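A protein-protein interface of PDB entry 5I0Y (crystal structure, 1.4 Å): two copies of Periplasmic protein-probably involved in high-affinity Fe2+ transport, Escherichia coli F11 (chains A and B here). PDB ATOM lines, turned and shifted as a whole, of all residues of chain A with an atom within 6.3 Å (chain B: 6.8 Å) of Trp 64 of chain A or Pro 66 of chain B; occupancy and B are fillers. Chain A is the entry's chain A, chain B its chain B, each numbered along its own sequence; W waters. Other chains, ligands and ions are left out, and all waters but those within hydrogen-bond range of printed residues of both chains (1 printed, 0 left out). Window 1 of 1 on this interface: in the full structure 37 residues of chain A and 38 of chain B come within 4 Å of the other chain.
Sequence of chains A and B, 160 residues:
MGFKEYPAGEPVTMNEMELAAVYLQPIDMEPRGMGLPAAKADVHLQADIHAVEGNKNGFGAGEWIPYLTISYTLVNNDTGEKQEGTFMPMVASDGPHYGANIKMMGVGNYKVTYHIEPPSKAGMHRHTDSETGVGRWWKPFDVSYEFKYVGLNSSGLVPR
The backbone NH (N) of Tyr 67 of chain A is in hydrogen-bond range of the side-chain hydroxyl (OH) of Tyr 67 of chain B (2.9 Å).
The backbone NH (N) of Tyr 67 of chain B lies within hydrogen-bond range of the side-chain hydroxyl (OH) of Tyr 98 of chain B, at 3.1 Å. The backbone NH (N) of Ala 51 of chain A lies within hydrogen-bond range of the backbone carbonyl oxygen (O) of Glu 63 of chain A. The side-chain hydroxyl of Tyr 98 of chain B sits at hydrogen-bond distance from the backbone NH of Leu 68 of chain B (3.0 Å). The backbone carbonyl oxygen (O) of Pro 119 of chain B lies within hydrogen-bond range of the backbone NH (N) of Met 124 of chain B (3.1 Å). The backbone carbonyl oxygen of Tyr 98 of chain A is in hydrogen-bond range of the backbone NH of Ala 47 of chain A. The side-chain hydroxyl of Tyr 98 of chain A lies within hydrogen-bond range of the backbone carbonyl oxygen of Ile 65 of chain A, at 2.6 Å.
Among the printed residues, pairs that only touch across the chains: Glu 63 of chain A with Pro 96 of chain B, Trp 64 of chain A with Pro 66 of chain B, Trp 64 of chain A with Tyr 67 of chain B, Trp 64 of chain A with Met 124 of chain B, Pro 66 of chain A with Trp 64 of chain B, Tyr 67 of chain A with Trp 64 of chain B, Tyr 67 of chain A with Tyr 98 of chain B, Pro 89 of chain A with Tyr 67 of chain B, Pro 89 of chain A with Met 124 of chain B, Met 90 of chain A with Met 124 of chain B and Tyr 98 of chain A with Tyr 67 of chain B.
Trp 64 of chain A touches just these residues of chain B: Pro 66, Tyr 67 and Met 124. Of chain A, only Trp 64 (3.9 Å) comes within 4 Å of Pro 66 of chain B. Printed residues of chain B within 4 Å of Tyr 67 of chain A: Trp 64, Tyr 67 and Tyr 98. Of the printed residues of chain A, Pro 96 of chain B touches Glu 63. Pro 118 of chain B touches none of the printed residues of chain A. The nearest residue of chain A that does not touch Pro 66 of chain B is Tyr 67 of chain A (4.2 Å). The nearest printed residue of chain B that does not touch Tyr 98 of chain A is Met 124 of chain B (7.0 Å).
Of the 16 printed residues of chain B, 6 touch a printed residue of chain A. Hydrophobic or aromatic side chains of chain B within 4 Å of the printed part of chain A: Trp 64, Pro 66, Tyr 67, Pro 96, Tyr 98 and Met 124. Hydrophobic or aromatic side chains of chain A within 4 Å of the printed part of chain B: Trp 64, Pro 66, Tyr 67, Pro 89 and Tyr 98. Among the printed residues, no Asp or Glu carboxylate lies within 4 Å of a Lys or Arg side-chain nitrogen of the other chain.
Glu 63 of chain A touches Pro 96 of chain B, but with the chains exchanged Pro 96 of chain A does not touch Glu 63 of chain B (4.9 Å). Trp 64 of chain A touches Tyr 67 of chain B, and with the chains exchanged Tyr 67 of chain A touches Trp 64 of chain B. Tyr 67 of chain B touches its own counterpart, Tyr 67 of chain A. Tyr 67 of chain A touches Tyr 98 of chain B, and with the chains exchanged Tyr 98 of chain A touches Tyr 67 of chain B. Positions printed for both chains: 49, 59, 63, 64, 65, 66, 67, 96 and 98. Of the 12 pairs that touch across the chains among the printed residues, 7 have their exchanged pair printed and touching as well.
Water W1 lies within hydrogen-bond range of the side-chain hydroxyl of Tyr 67 of chain A and the backbone carbonyl oxygen of Leu 68 of chain B.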
ATOM      1  N   ALA A  47      19.567 -11.485  26.829  1.00  0.00           N
ATOM      2  CA  ALA A  47      20.838 -11.304  27.553  1.00  0.00           C
ATOM      3  C   ALA A  47      21.886 -10.855  26.538  1.00  0.00           C
ATOM      4  O   ALA A  47      22.101 -11.532  25.521  1.00  0.00           O
ATOM      5  CB  ALA A  47      21.250 -12.595  28.215  1.00  0.00           C
ATOM      6  N   ASP A  48      22.495  -9.699  26.793  1.00  0.00           N
ATOM      7  CA  ASP A  48      23.590  -9.138  25.981  1.00  0.00           C
ATOM      8  C   ASP A  48      24.886  -9.358  26.723  1.00  0.00           C
ATOM      9  O   ASP A  48      25.085  -8.796  27.803  1.00  0.00           O
ATOM     10  CB  ASP A  48      23.394  -7.639  25.753  1.00  0.00           C
ATOM     11  CG  ASP A  48      22.331  -7.338  24.740  1.00  0.00           C
ATOM     12  OD1 ASP A  48      22.082  -8.190  23.854  1.00  0.00           O
ATOM     13  OD2 ASP A  48      21.774  -6.229  24.820  1.00  0.00           O
ATOM     14  N   ILE A  49      25.754 -10.188  26.157  1.00  0.00           N
ATOM     15  CA  ILE A  49      26.930 -10.666  26.879  1.00  0.00           C
ATOM     16  C   ILE A  49      28.137 -10.604  25.953  1.00  0.00           C
ATOM     17  O   ILE A  49      28.204 -11.306  24.961  1.00  0.00           O
ATOM     18  CB  ILE A  49      26.756 -12.105  27.407  1.00  0.00           C
ATOM     19  CG1 ILE A  49      25.530 -12.181  28.342  1.00  0.00           C
ATOM     20  CG2 ILE A  49      28.022 -12.541  28.153  1.00  0.00           C
ATOM     21  CD1 ILE A  49      25.113 -13.577  28.727  1.00  0.00           C
ATOM     22  N   HIS A  50      29.088  -9.753  26.304  1.00  0.00           N
ATOM     23  CA  HIS A  50      30.297  -9.540  25.516  1.00  0.00           C
ATOM     24  C   HIS A  50      31.488  -9.485  26.401  1.00  0.00           C
ATOM     25  O   HIS A  50      31.388  -9.056  27.546  1.00  0.00           O
ATOM     26  CB  HIS A  50      30.183  -8.253  24.709  1.00  0.00           C
ATOM     27  CG  HIS A  50      29.010  -8.264  23.772  1.00  0.00           C
ATOM     28  ND1 HIS A  50      27.765  -7.960  24.172  1.00  0.00           N
ATOM     29  CD2 HIS A  50      28.917  -8.633  22.437  1.00  0.00           C
ATOM     30  CE1 HIS A  50      26.916  -8.108  23.134  1.00  0.00           C
ATOM     31  NE2 HIS A  50      27.622  -8.527  22.080  1.00  0.00           N
ATOM     32  N   ALA A  51      32.640  -9.913  25.893  1.00  0.00           N
ATOM     33  CA  ALA A  51      33.882  -9.806  26.659  1.00  0.00           C
ATOM     34  C   ALA A  51      34.221  -8.348  26.922  1.00  0.00           C
ATOM     35  O   ALA A  51      33.847  -7.456  26.163  1.00  0.00           O
ATOM     36  CB  ALA A  51      35.028 -10.475  25.910  1.00  0.00           C
ATOM     37  N   PHE A  59      38.615 -14.360  24.337  1.00  0.00           N
ATOM     38  CA  PHE A  59      37.740 -13.382  23.675  1.00  0.00           C
ATOM     39  C   PHE A  59      38.243 -11.945  23.803  1.00  0.00           C
ATOM     40  O   PHE A  59      38.598 -11.503  24.898  1.00  0.00           O
ATOM     41  CB  PHE A  59      36.292 -13.532  24.191  1.00  0.00           C
ATOM     42  CG  PHE A  59      35.726 -14.903  23.954  1.00  0.00           C
ATOM     43  CD1 PHE A  59      35.286 -15.289  22.691  1.00  0.00           C
ATOM     44  CD2 PHE A  59      35.687 -15.846  24.981  1.00  0.00           C
ATOM     45  CE1 PHE A  59      34.802 -16.582  22.473  1.00  0.00           C
ATOM     46  CE2 PHE A  59      35.192 -17.126  24.768  1.00  0.00           C
ATOM     47  CZ  PHE A  59      34.760 -17.501  23.510  1.00  0.00           C
ATOM     48  N   GLY A  60      38.293 -11.226  22.688  1.00  0.00           N
ATOM     49  CA  GLY A  60      38.708  -9.828  22.723  1.00  0.00           C
ATOM     50  C   GLY A  60      37.601  -8.883  23.173  1.00  0.00           C
ATOM     51  O   GLY A  60      36.404  -9.229  23.128  1.00  0.00           O
ATOM     52  N   GLY A  62      34.655  -6.551  23.565  1.00  0.00           N
ATOM     53  CA  GLY A  62      33.472  -6.324  22.752  1.00  0.00           C
ATOM     54  C   GLY A  62      32.941  -7.550  22.015  1.00  0.00           C
ATOM     55  O   GLY A  62      31.866  -7.493  21.415  1.00  0.00           O
ATOM     56  N   GLU A  63      33.687  -8.648  22.041  1.00  0.00           N
ATOM     57  CA  GLU A  63      33.282  -9.831  21.296  1.00  0.00           C
ATOM     58  C   GLU A  63      32.121 -10.523  22.003  1.00  0.00           C
ATOM     59  O   GLU A  63      32.103 -10.603  23.229  1.00  0.00           O
ATOM     60  CB  GLU A  63      34.460 -10.787  21.162  1.00  0.00           C
ATOM     61  CG  GLU A  63      34.228 -11.974  20.257  1.00  0.00           C
ATOM     62  CD  GLU A  63      35.498 -12.740  19.952  1.00  0.00           C
ATOM     63  OE1 GLU A  63      36.606 -12.248  20.292  1.00  0.00           O
ATOM     64  OE2 GLU A  63      35.373 -13.836  19.364  1.00  0.00           O
ATOM     65  N   TRP A  64      31.169 -11.025  21.226  1.00  0.00           N
ATOM     66  CA  TRP A  64      30.105 -11.850  21.753  1.00  0.00           C
ATOM     67  C   TRP A  64      30.662 -13.092  22.383  1.00  0.00           C
ATOM     68  O   TRP A  64      31.623 -13.684  21.876  1.00  0.00           O
ATOM     69  CB  TRP A  64      29.180 -12.236  20.612  1.00  0.00           C
ATOM     70  CG  TRP A  64      27.911 -12.872  21.116  1.00  0.00           C
ATOM     71  CD1 TRP A  64      27.032 -12.358  22.078  1.00  0.00           C
ATOM     72  CD2 TRP A  64      27.326 -14.137  20.680  1.00  0.00           C
ATOM     73  NE1 TRP A  64      25.980 -13.225  22.273  1.00  0.00           N
ATOM     74  CE2 TRP A  64      26.087 -14.296  21.432  1.00  0.00           C
ATOM     75  CE3 TRP A  64      27.674 -15.105  19.742  1.00  0.00           C
ATOM     76  CZ2 TRP A  64      25.273 -15.401  21.278  1.00  0.00           C
ATOM     77  CZ3 TRP A  64      26.834 -16.213  19.587  1.00  0.00           C
ATOM     78  CH2 TRP A  64      25.651 -16.349  20.326  1.00  0.00           C
ATOM     79  N   ILE A  65      30.082 -13.522  23.500  1.00  0.00           N
ATOM     80  CA  ILE A  65      30.478 -14.789  24.098  1.00  0.00           C
ATOM     81  C   ILE A  65      29.494 -15.837  23.615  1.00  0.00           C
ATOM     82  O   ILE A  65      28.330 -15.818  24.022  1.00  0.00           O
ATOM     83  CB  ILE A  65      30.463 -14.743  25.642  1.00  0.00           C
ATOM     84  CG1 ILE A  65      31.268 -13.526  26.159  1.00  0.00           C
ATOM     85  CG2 ILE A  65      30.924 -16.084  26.187  1.00  0.00           C
ATOM     86  CD1 ILE A  65      32.777 -13.565  25.884  1.00  0.00           C
ATOM     87  N   PRO A  66      29.960 -16.771  22.781  1.00  0.00           N
ATOM     88  CA  PRO A  66      29.087 -17.750  22.162  1.00  0.00           C
ATOM     89  C   PRO A  66      29.024 -19.009  22.992  1.00  0.00           C
ATOM     90  O   PRO A  66      29.826 -19.176  23.919  1.00  0.00           O
ATOM     91  CB  PRO A  66      29.813 -18.033  20.845  1.00  0.00           C
ATOM     92  CG  PRO A  66      31.272 -17.985  21.250  1.00  0.00           C
ATOM     93  CD  PRO A  66      31.363 -16.932  22.335  1.00  0.00           C
ATOM     94  N   TYR A  67      28.074 -19.882  22.682  1.00  0.00           N
ATOM     95  CA  TYR A  67      27.972 -21.221  23.281  1.00  0.00           C
ATOM     96  C   TYR A  67      27.624 -21.206  24.769  1.00  0.00           C
ATOM     97  O   TYR A  67      27.845 -22.188  25.445  1.00  0.00           O
ATOM     98  CB  TYR A  67      29.216 -22.091  22.999  1.00  0.00           C
ATOM     99  CG  TYR A  67      29.312 -22.488  21.546  1.00  0.00           C
ATOM    100  CD1 TYR A  67      28.710 -23.653  21.068  1.00  0.00           C
ATOM    101  CD2 TYR A  67      29.983 -21.680  20.640  1.00  0.00           C
ATOM    102  CE1 TYR A  67      28.791 -24.003  19.724  1.00  0.00           C
ATOM    103  CE2 TYR A  67      30.075 -22.027  19.298  1.00  0.00           C
ATOM    104  CZ  TYR A  67      29.482 -23.170  18.853  1.00  0.00           C
ATOM    105  OH  TYR A  67      29.616 -23.452  17.508  1.00  0.00           O
ATOM    106  N   PRO A  89      20.356 -19.348  21.765  1.00  0.00           N
ATOM    107  CA  PRO A  89      21.214 -18.467  20.976  1.00  0.00           C
ATOM    108  C   PRO A  89      20.472 -18.000  19.726  1.00  0.00           C
ATOM    109  O   PRO A  89      19.783 -18.798  19.084  1.00  0.00           O
ATOM    110  CB  PRO A  89      22.407 -19.350  20.584  1.00  0.00           C
ATOM    111  CG  PRO A  89      22.104 -20.725  21.084  1.00  0.00           C
ATOM    112  CD  PRO A  89      20.704 -20.769  21.606  1.00  0.00           C
ATOM    113  N   MET A  90      20.616 -16.729  19.400  1.00  0.00           N
ATOM    114  CA  MET A  90      19.845 -16.133  18.312  1.00  0.00           C
ATOM    115  C   MET A  90      20.691 -15.138  17.570  1.00  0.00           C
ATOM    116  O   MET A  90      21.732 -14.692  18.067  1.00  0.00           O
ATOM    117  CB  MET A  90      18.637 -15.385  18.869  1.00  0.00           C
ATOM    118  CG  MET A  90      17.811 -16.195  19.850  1.00  0.00           C
ATOM    119  SD  MET A  90      16.220 -15.405  20.183  1.00  0.00           S
ATOM    120  CE  MET A  90      15.335 -16.029  18.774  1.00  0.00           C
ATOM    121  N   PRO A  96      24.299 -11.272  17.172  1.00  0.00           N
ATOM    122  CA  PRO A  96      23.890 -12.396  18.016  1.00  0.00           C
ATOM    123  C   PRO A  96      23.557 -11.978  19.448  1.00  0.00           C
ATOM    124  O   PRO A  96      24.111 -11.004  19.985  1.00  0.00           O
ATOM    125  CB  PRO A  96      25.113 -13.307  17.993  1.00  0.00           C
ATOM    126  CG  PRO A  96      26.265 -12.379  17.749  1.00  0.00           C
ATOM    127  CD  PRO A  96      25.737 -11.309  16.842  1.00  0.00           C
ATOM    128  N   HIS A  97      22.646 -12.729  20.050  1.00  0.00           N
ATOM    129  CA  HIS A  97      22.309 -12.571  21.475  1.00  0.00           C
ATOM    130  C   HIS A  97      21.715 -13.862  21.966  1.00  0.00           C
ATOM    131  O   HIS A  97      21.635 -14.850  21.225  1.00  0.00           O
ATOM    132  CB  HIS A  97      21.338 -11.411  21.697  1.00  0.00           C
ATOM    133  CG  HIS A  97      20.014 -11.610  21.024  1.00  0.00           C
ATOM    134  ND1 HIS A  97      19.638 -10.898  19.925  1.00  0.00           N
ATOM    135  CD2 HIS A  97      18.972 -12.490  21.304  1.00  0.00           C
ATOM    136  CE1 HIS A  97      18.403 -11.297  19.543  1.00  0.00           C
ATOM    137  NE2 HIS A  97      17.987 -12.259  20.376  1.00  0.00           N
ATOM    138  N   TYR A  98      21.286 -13.871  23.229  1.00  0.00           N
ATOM    139  CA  TYR A  98      20.512 -14.966  23.798  1.00  0.00           C
ATOM    140  C   TYR A  98      19.174 -14.403  24.204  1.00  0.00           C
ATOM    141  O   TYR A  98      19.107 -13.307  24.728  1.00  0.00           O
ATOM    142  CB  TYR A  98      21.210 -15.573  25.034  1.00  0.00           C
ATOM    143  CG  TYR A  98      22.586 -16.122  24.733  1.00  0.00           C
ATOM    144  CD1 TYR A  98      22.748 -17.421  24.281  1.00  0.00           C
ATOM    145  CD2 TYR A  98      23.715 -15.312  24.888  1.00  0.00           C
ATOM    146  CE1 TYR A  98      24.016 -17.922  23.994  1.00  0.00           C
ATOM    147  CE2 TYR A  98      24.993 -15.806  24.602  1.00  0.00           C
ATOM    148  CZ  TYR A  98      25.137 -17.095  24.162  1.00  0.00           C
ATOM    149  OH  TYR A  98      26.397 -17.588  23.883  1.00  0.00           O
ATOM    150  N   ILE B  49      36.670 -18.986   9.852  1.00  0.00           N
ATOM    151  CA  ILE B  49      35.471 -18.502   9.160  1.00  0.00           C
ATOM    152  C   ILE B  49      34.922 -17.244   9.826  1.00  0.00           C
ATOM    153  O   ILE B  49      34.536 -17.256  10.994  1.00  0.00           O
ATOM    154  CB  ILE B  49      34.387 -19.598   9.083  1.00  0.00           C
ATOM    155  CG1 ILE B  49      34.918 -20.843   8.347  1.00  0.00           C
ATOM    156  CG2 ILE B  49      33.145 -19.051   8.386  1.00  0.00           C
ATOM    157  CD1 ILE B  49      34.064 -22.075   8.519  1.00  0.00           C
ATOM    158  N   PHE B  59      25.806 -10.659  10.878  1.00  0.00           N
ATOM    159  CA  PHE B  59      27.194 -10.581  11.351  1.00  0.00           C
ATOM    160  C   PHE B  59      27.965  -9.456  10.679  1.00  0.00           C
ATOM    161  O   PHE B  59      27.876  -9.271   9.471  1.00  0.00           O
ATOM    162  CB  PHE B  59      27.907 -11.934  11.152  1.00  0.00           C
ATOM    163  CG  PHE B  59      27.226 -13.067  11.856  1.00  0.00           C
ATOM    164  CD1 PHE B  59      27.408 -13.275  13.226  1.00  0.00           C
ATOM    165  CD2 PHE B  59      26.342 -13.887  11.162  1.00  0.00           C
ATOM    166  CE1 PHE B  59      26.731 -14.297  13.885  1.00  0.00           C
ATOM    167  CE2 PHE B  59      25.680 -14.911  11.813  1.00  0.00           C
ATOM    168  CZ  PHE B  59      25.874 -15.114  13.169  1.00  0.00           C
ATOM    169  N   GLU B  63      33.590 -10.643  12.048  1.00  0.00           N
ATOM    170  CA  GLU B  63      33.048 -11.406  13.160  1.00  0.00           C
ATOM    171  C   GLU B  63      33.040 -12.897  12.895  1.00  0.00           C
ATOM    172  O   GLU B  63      32.738 -13.341  11.797  1.00  0.00           O
ATOM    173  CB  GLU B  63      31.655 -10.881  13.510  1.00  0.00           C
ATOM    174  CG  GLU B  63      31.707  -9.489  14.142  1.00  0.00           C
ATOM    175  CD  GLU B  63      30.368  -8.789  14.229  1.00  0.00           C
ATOM    176  OE1 GLU B  63      30.396  -7.552  14.475  1.00  0.00           O
ATOM    177  OE2 GLU B  63      29.312  -9.468  14.079  1.00  0.00           O
ATOM    178  N   TRP B  64      33.391 -13.662  13.912  1.00  0.00           N
ATOM    179  CA  TRP B  64      33.332 -15.108  13.819  1.00  0.00           C
ATOM    180  C   TRP B  64      31.933 -15.583  13.514  1.00  0.00           C
ATOM    181  O   TRP B  64      30.943 -14.995  13.959  1.00  0.00           O
ATOM    182  CB  TRP B  64      33.796 -15.712  15.136  1.00  0.00           C
ATOM    183  CG  TRP B  64      33.997 -17.191  15.080  1.00  0.00           C
ATOM    184  CD1 TRP B  64      34.749 -17.901  14.155  1.00  0.00           C
ATOM    185  CD2 TRP B  64      33.436 -18.191  15.971  1.00  0.00           C
ATOM    186  NE1 TRP B  64      34.713 -19.234  14.408  1.00  0.00           N
ATOM    187  CE2 TRP B  64      33.938 -19.485  15.498  1.00  0.00           C
ATOM    188  CE3 TRP B  64      32.615 -18.155  17.090  1.00  0.00           C
ATOM    189  CZ2 TRP B  64      33.635 -20.678  16.141  1.00  0.00           C
ATOM    190  CZ3 TRP B  64      32.306 -19.376  17.723  1.00  0.00           C
ATOM    191  CH2 TRP B  64      32.790 -20.598  17.252  1.00  0.00           C
ATOM    192  N   ILE B  65      31.815 -16.635  12.715  1.00  0.00           N
ATOM    193  CA  ILE B  65      30.490 -17.207  12.484  1.00  0.00           C
ATOM    194  C   ILE B  65      30.347 -18.408  13.426  1.00  0.00           C
ATOM    195  O   ILE B  65      31.024 -19.410  13.244  1.00  0.00           O
ATOM    196  CB  ILE B  65      30.318 -17.658  11.025  1.00  0.00           C
ATOM    197  CG1 ILE B  65      30.587 -16.500  10.033  1.00  0.00           C
ATOM    198  CG2 ILE B  65      28.921 -18.243  10.838  1.00  0.00           C
ATOM    199  CD1 ILE B  65      29.661 -15.297  10.138  1.00  0.00           C
ATOM    200  N   PRO B  66      29.475 -18.298  14.449  1.00  0.00           N
ATOM    201  CA  PRO B  66      29.308 -19.352  15.456  1.00  0.00           C
ATOM    202  C   PRO B  66      28.265 -20.382  15.058  1.00  0.00           C
ATOM    203  O   PRO B  66      27.514 -20.169  14.095  1.00  0.00           O
ATOM    204  CB  PRO B  66      28.825 -18.556  16.675  1.00  0.00           C
ATOM    205  CG  PRO B  66      27.923 -17.513  16.068  1.00  0.00           C
ATOM    206  CD  PRO B  66      28.569 -17.161  14.724  1.00  0.00           C
ATOM    207  N   TYR B  67      28.246 -21.507  15.769  1.00  0.00           N
ATOM    208  CA  TYR B  67      27.201 -22.550  15.622  1.00  0.00           C
ATOM    209  C   TYR B  67      27.226 -23.269  14.282  1.00  0.00           C
ATOM    210  O   TYR B  67      26.231 -23.892  13.903  1.00  0.00           O
ATOM    211  CB  TYR B  67      25.795 -22.004  15.945  1.00  0.00           C
ATOM    212  CG  TYR B  67      25.702 -21.596  17.386  1.00  0.00           C
ATOM    213  CD1 TYR B  67      25.388 -22.528  18.378  1.00  0.00           C
ATOM    214  CD2 TYR B  67      25.942 -20.282  17.757  1.00  0.00           C
ATOM    215  CE1 TYR B  67      25.310 -22.141  19.715  1.00  0.00           C
ATOM    216  CE2 TYR B  67      25.876 -19.894  19.086  1.00  0.00           C
ATOM    217  CZ  TYR B  67      25.567 -20.818  20.043  1.00  0.00           C
ATOM    218  OH  TYR B  67      25.509 -20.377  21.349  1.00  0.00           O
ATOM    219  N   LEU B  68      28.365 -23.251  13.593  1.00  0.00           N
ATOM    220  CA  LEU B  68      28.464 -24.024  12.351  1.00  0.00           C
ATOM    221  C   LEU B  68      28.696 -25.504  12.655  1.00  0.00           C
ATOM    222  O   LEU B  68      29.180 -25.868  13.727  1.00  0.00           O
ATOM    223  CB  LEU B  68      29.599 -23.499  11.472  1.00  0.00           C
ATOM    224  CG  LEU B  68      29.403 -22.070  10.970  1.00  0.00           C
ATOM    225  CD1 LEU B  68      30.617 -21.609  10.178  1.00  0.00           C
ATOM    226  CD2 LEU B  68      28.141 -21.906  10.133  1.00  0.00           C
ATOM    227  N   THR B  69      28.362 -26.371  11.694  1.00  0.00           N
ATOM    228  CA  THR B  69      28.674 -27.788  11.759  1.00  0.00           C
ATOM    229  C   THR B  69      29.564 -28.064  10.556  1.00  0.00           C
ATOM    230  O   THR B  69      29.190 -27.803   9.409  1.00  0.00           O
ATOM    231  CB  THR B  69      27.393 -28.611  11.687  1.00  0.00           C
ATOM    232  OG1 THR B  69      26.561 -28.212  12.783  1.00  0.00           O
ATOM    233  CG2 THR B  69      27.702 -30.111  11.791  1.00  0.00           C
ATOM    234  N   PRO B  96      37.980 -17.776  18.875  1.00  0.00           N
ATOM    235  CA  PRO B  96      37.273 -19.024  18.551  1.00  0.00           C
ATOM    236  C   PRO B  96      37.553 -19.510  17.137  1.00  0.00           C
ATOM    237  O   PRO B  96      37.877 -18.713  16.256  1.00  0.00           O
ATOM    238  CB  PRO B  96      35.798 -18.612  18.677  1.00  0.00           C
ATOM    239  CG  PRO B  96      35.793 -17.149  18.399  1.00  0.00           C
ATOM    240  CD  PRO B  96      37.079 -16.615  18.986  1.00  0.00           C
ATOM    241  N   TYR B  98      36.952 -23.456  14.447  1.00  0.00           N
ATOM    242  CA  TYR B  98      36.543 -24.867  14.403  1.00  0.00           C
ATOM    243  C   TYR B  98      37.758 -25.712  14.089  1.00  0.00           C
ATOM    244  O   TYR B  98      38.561 -25.329  13.250  1.00  0.00           O
ATOM    245  CB  TYR B  98      35.448 -25.106  13.345  1.00  0.00           C
ATOM    246  CG  TYR B  98      34.230 -24.245  13.563  1.00  0.00           C
ATOM    247  CD1 TYR B  98      33.186 -24.683  14.386  1.00  0.00           C
ATOM    248  CD2 TYR B  98      34.130 -23.003  12.956  1.00  0.00           C
ATOM    249  CE1 TYR B  98      32.067 -23.889  14.590  1.00  0.00           C
ATOM    250  CE2 TYR B  98      33.012 -22.192  13.153  1.00  0.00           C
ATOM    251  CZ  TYR B  98      31.988 -22.641  13.978  1.00  0.00           C
ATOM    252  OH  TYR B  98      30.886 -21.835  14.179  1.00  0.00           O
ATOM    253  N   PRO B 118      24.745 -24.543   8.095  1.00  0.00           N
ATOM    254  CA  PRO B 118      24.511 -23.252   8.733  1.00  0.00           C
ATOM    255  C   PRO B 118      24.123 -23.358  10.214  1.00  0.00           C
ATOM    256  O   PRO B 118      23.807 -24.441  10.706  1.00  0.00           O
ATOM    257  CB  PRO B 118      23.372 -22.644   7.895  1.00  0.00           C
ATOM    258  CG  PRO B 118      22.615 -23.850   7.437  1.00  0.00           C
ATOM    259  CD  PRO B 118      23.675 -24.866   7.127  1.00  0.00           C
ATOM    260  N   PRO B 119      24.140 -22.216  10.908  1.00  0.00           N
ATOM    261  CA  PRO B 119      23.927 -22.187  12.357  1.00  0.00           C
ATOM    262  C   PRO B 119      22.585 -22.744  12.827  1.00  0.00           C
ATOM    263  O   PRO B 119      22.480 -23.160  13.980  1.00  0.00           O
ATOM    264  CB  PRO B 119      24.072 -20.701  12.688  1.00  0.00           C
ATOM    265  CG  PRO B 119      25.034 -20.209  11.659  1.00  0.00           C
ATOM    266  CD  PRO B 119      24.587 -20.901  10.409  1.00  0.00           C
ATOM    267  N   ALA B 122      22.862 -26.398  14.493  1.00  0.00           N
ATOM    268  CA  ALA B 122      23.407 -26.562  15.839  1.00  0.00           C
ATOM    269  C   ALA B 122      22.639 -25.758  16.875  1.00  0.00           C
ATOM    270  O   ALA B 122      23.051 -25.700  18.034  1.00  0.00           O
ATOM    271  CB  ALA B 122      24.900 -26.199  15.864  1.00  0.00           C
ATOM    272  N   MET B 124      21.213 -22.309  16.663  1.00  0.00           N
ATOM    273  CA  MET B 124      21.084 -20.861  16.656  1.00  0.00           C
ATOM    274  C   MET B 124      19.838 -20.500  15.857  1.00  0.00           C
ATOM    275  O   MET B 124      19.612 -21.055  14.776  1.00  0.00           O
ATOM    276  CB  MET B 124      22.326 -20.167  16.089  1.00  0.00           C
ATOM    277  CG  MET B 124      22.145 -18.668  15.899  1.00  0.00           C
ATOM    278  SD  MET B 124      23.654 -17.817  15.438  1.00  0.00           S
ATOM    279  CE  MET B 124      24.172 -17.196  17.041  1.00  0.00           C
ATOM    280  N   TRP B 137      19.139 -18.391   5.994  1.00  0.00           N
ATOM    281  CA  TRP B 137      20.425 -19.074   5.885  1.00  0.00           C
ATOM    282  C   TRP B 137      20.658 -19.577   4.506  1.00  0.00           C
ATOM    283  O   TRP B 137      19.728 -20.007   3.817  1.00  0.00           O
ATOM    284  CB  TRP B 137      20.551 -20.238   6.858  1.00  0.00           C
ATOM    285  CG  TRP B 137      20.556 -19.811   8.284  1.00  0.00           C
ATOM    286  CD1 TRP B 137      19.615 -20.126   9.257  1.00  0.00           C
ATOM    287  CD2 TRP B 137      21.543 -18.966   8.953  1.00  0.00           C
ATOM    288  NE1 TRP B 137      19.940 -19.539  10.447  1.00  0.00           N
ATOM    289  CE2 TRP B 137      21.091 -18.842  10.342  1.00  0.00           C
ATOM    290  CE3 TRP B 137      22.722 -18.341   8.562  1.00  0.00           C
ATOM    291  CZ2 TRP B 137      21.800 -18.104  11.280  1.00  0.00           C
ATOM    292  CZ3 TRP B 137      23.423 -17.594   9.519  1.00  0.00           C
ATOM    293  CH2 TRP B 137      22.970 -17.481  10.842  1.00  0.00           C
HETATM  294  O   HOH W   1      28.467 -25.471  16.460  1.00  0.00           O
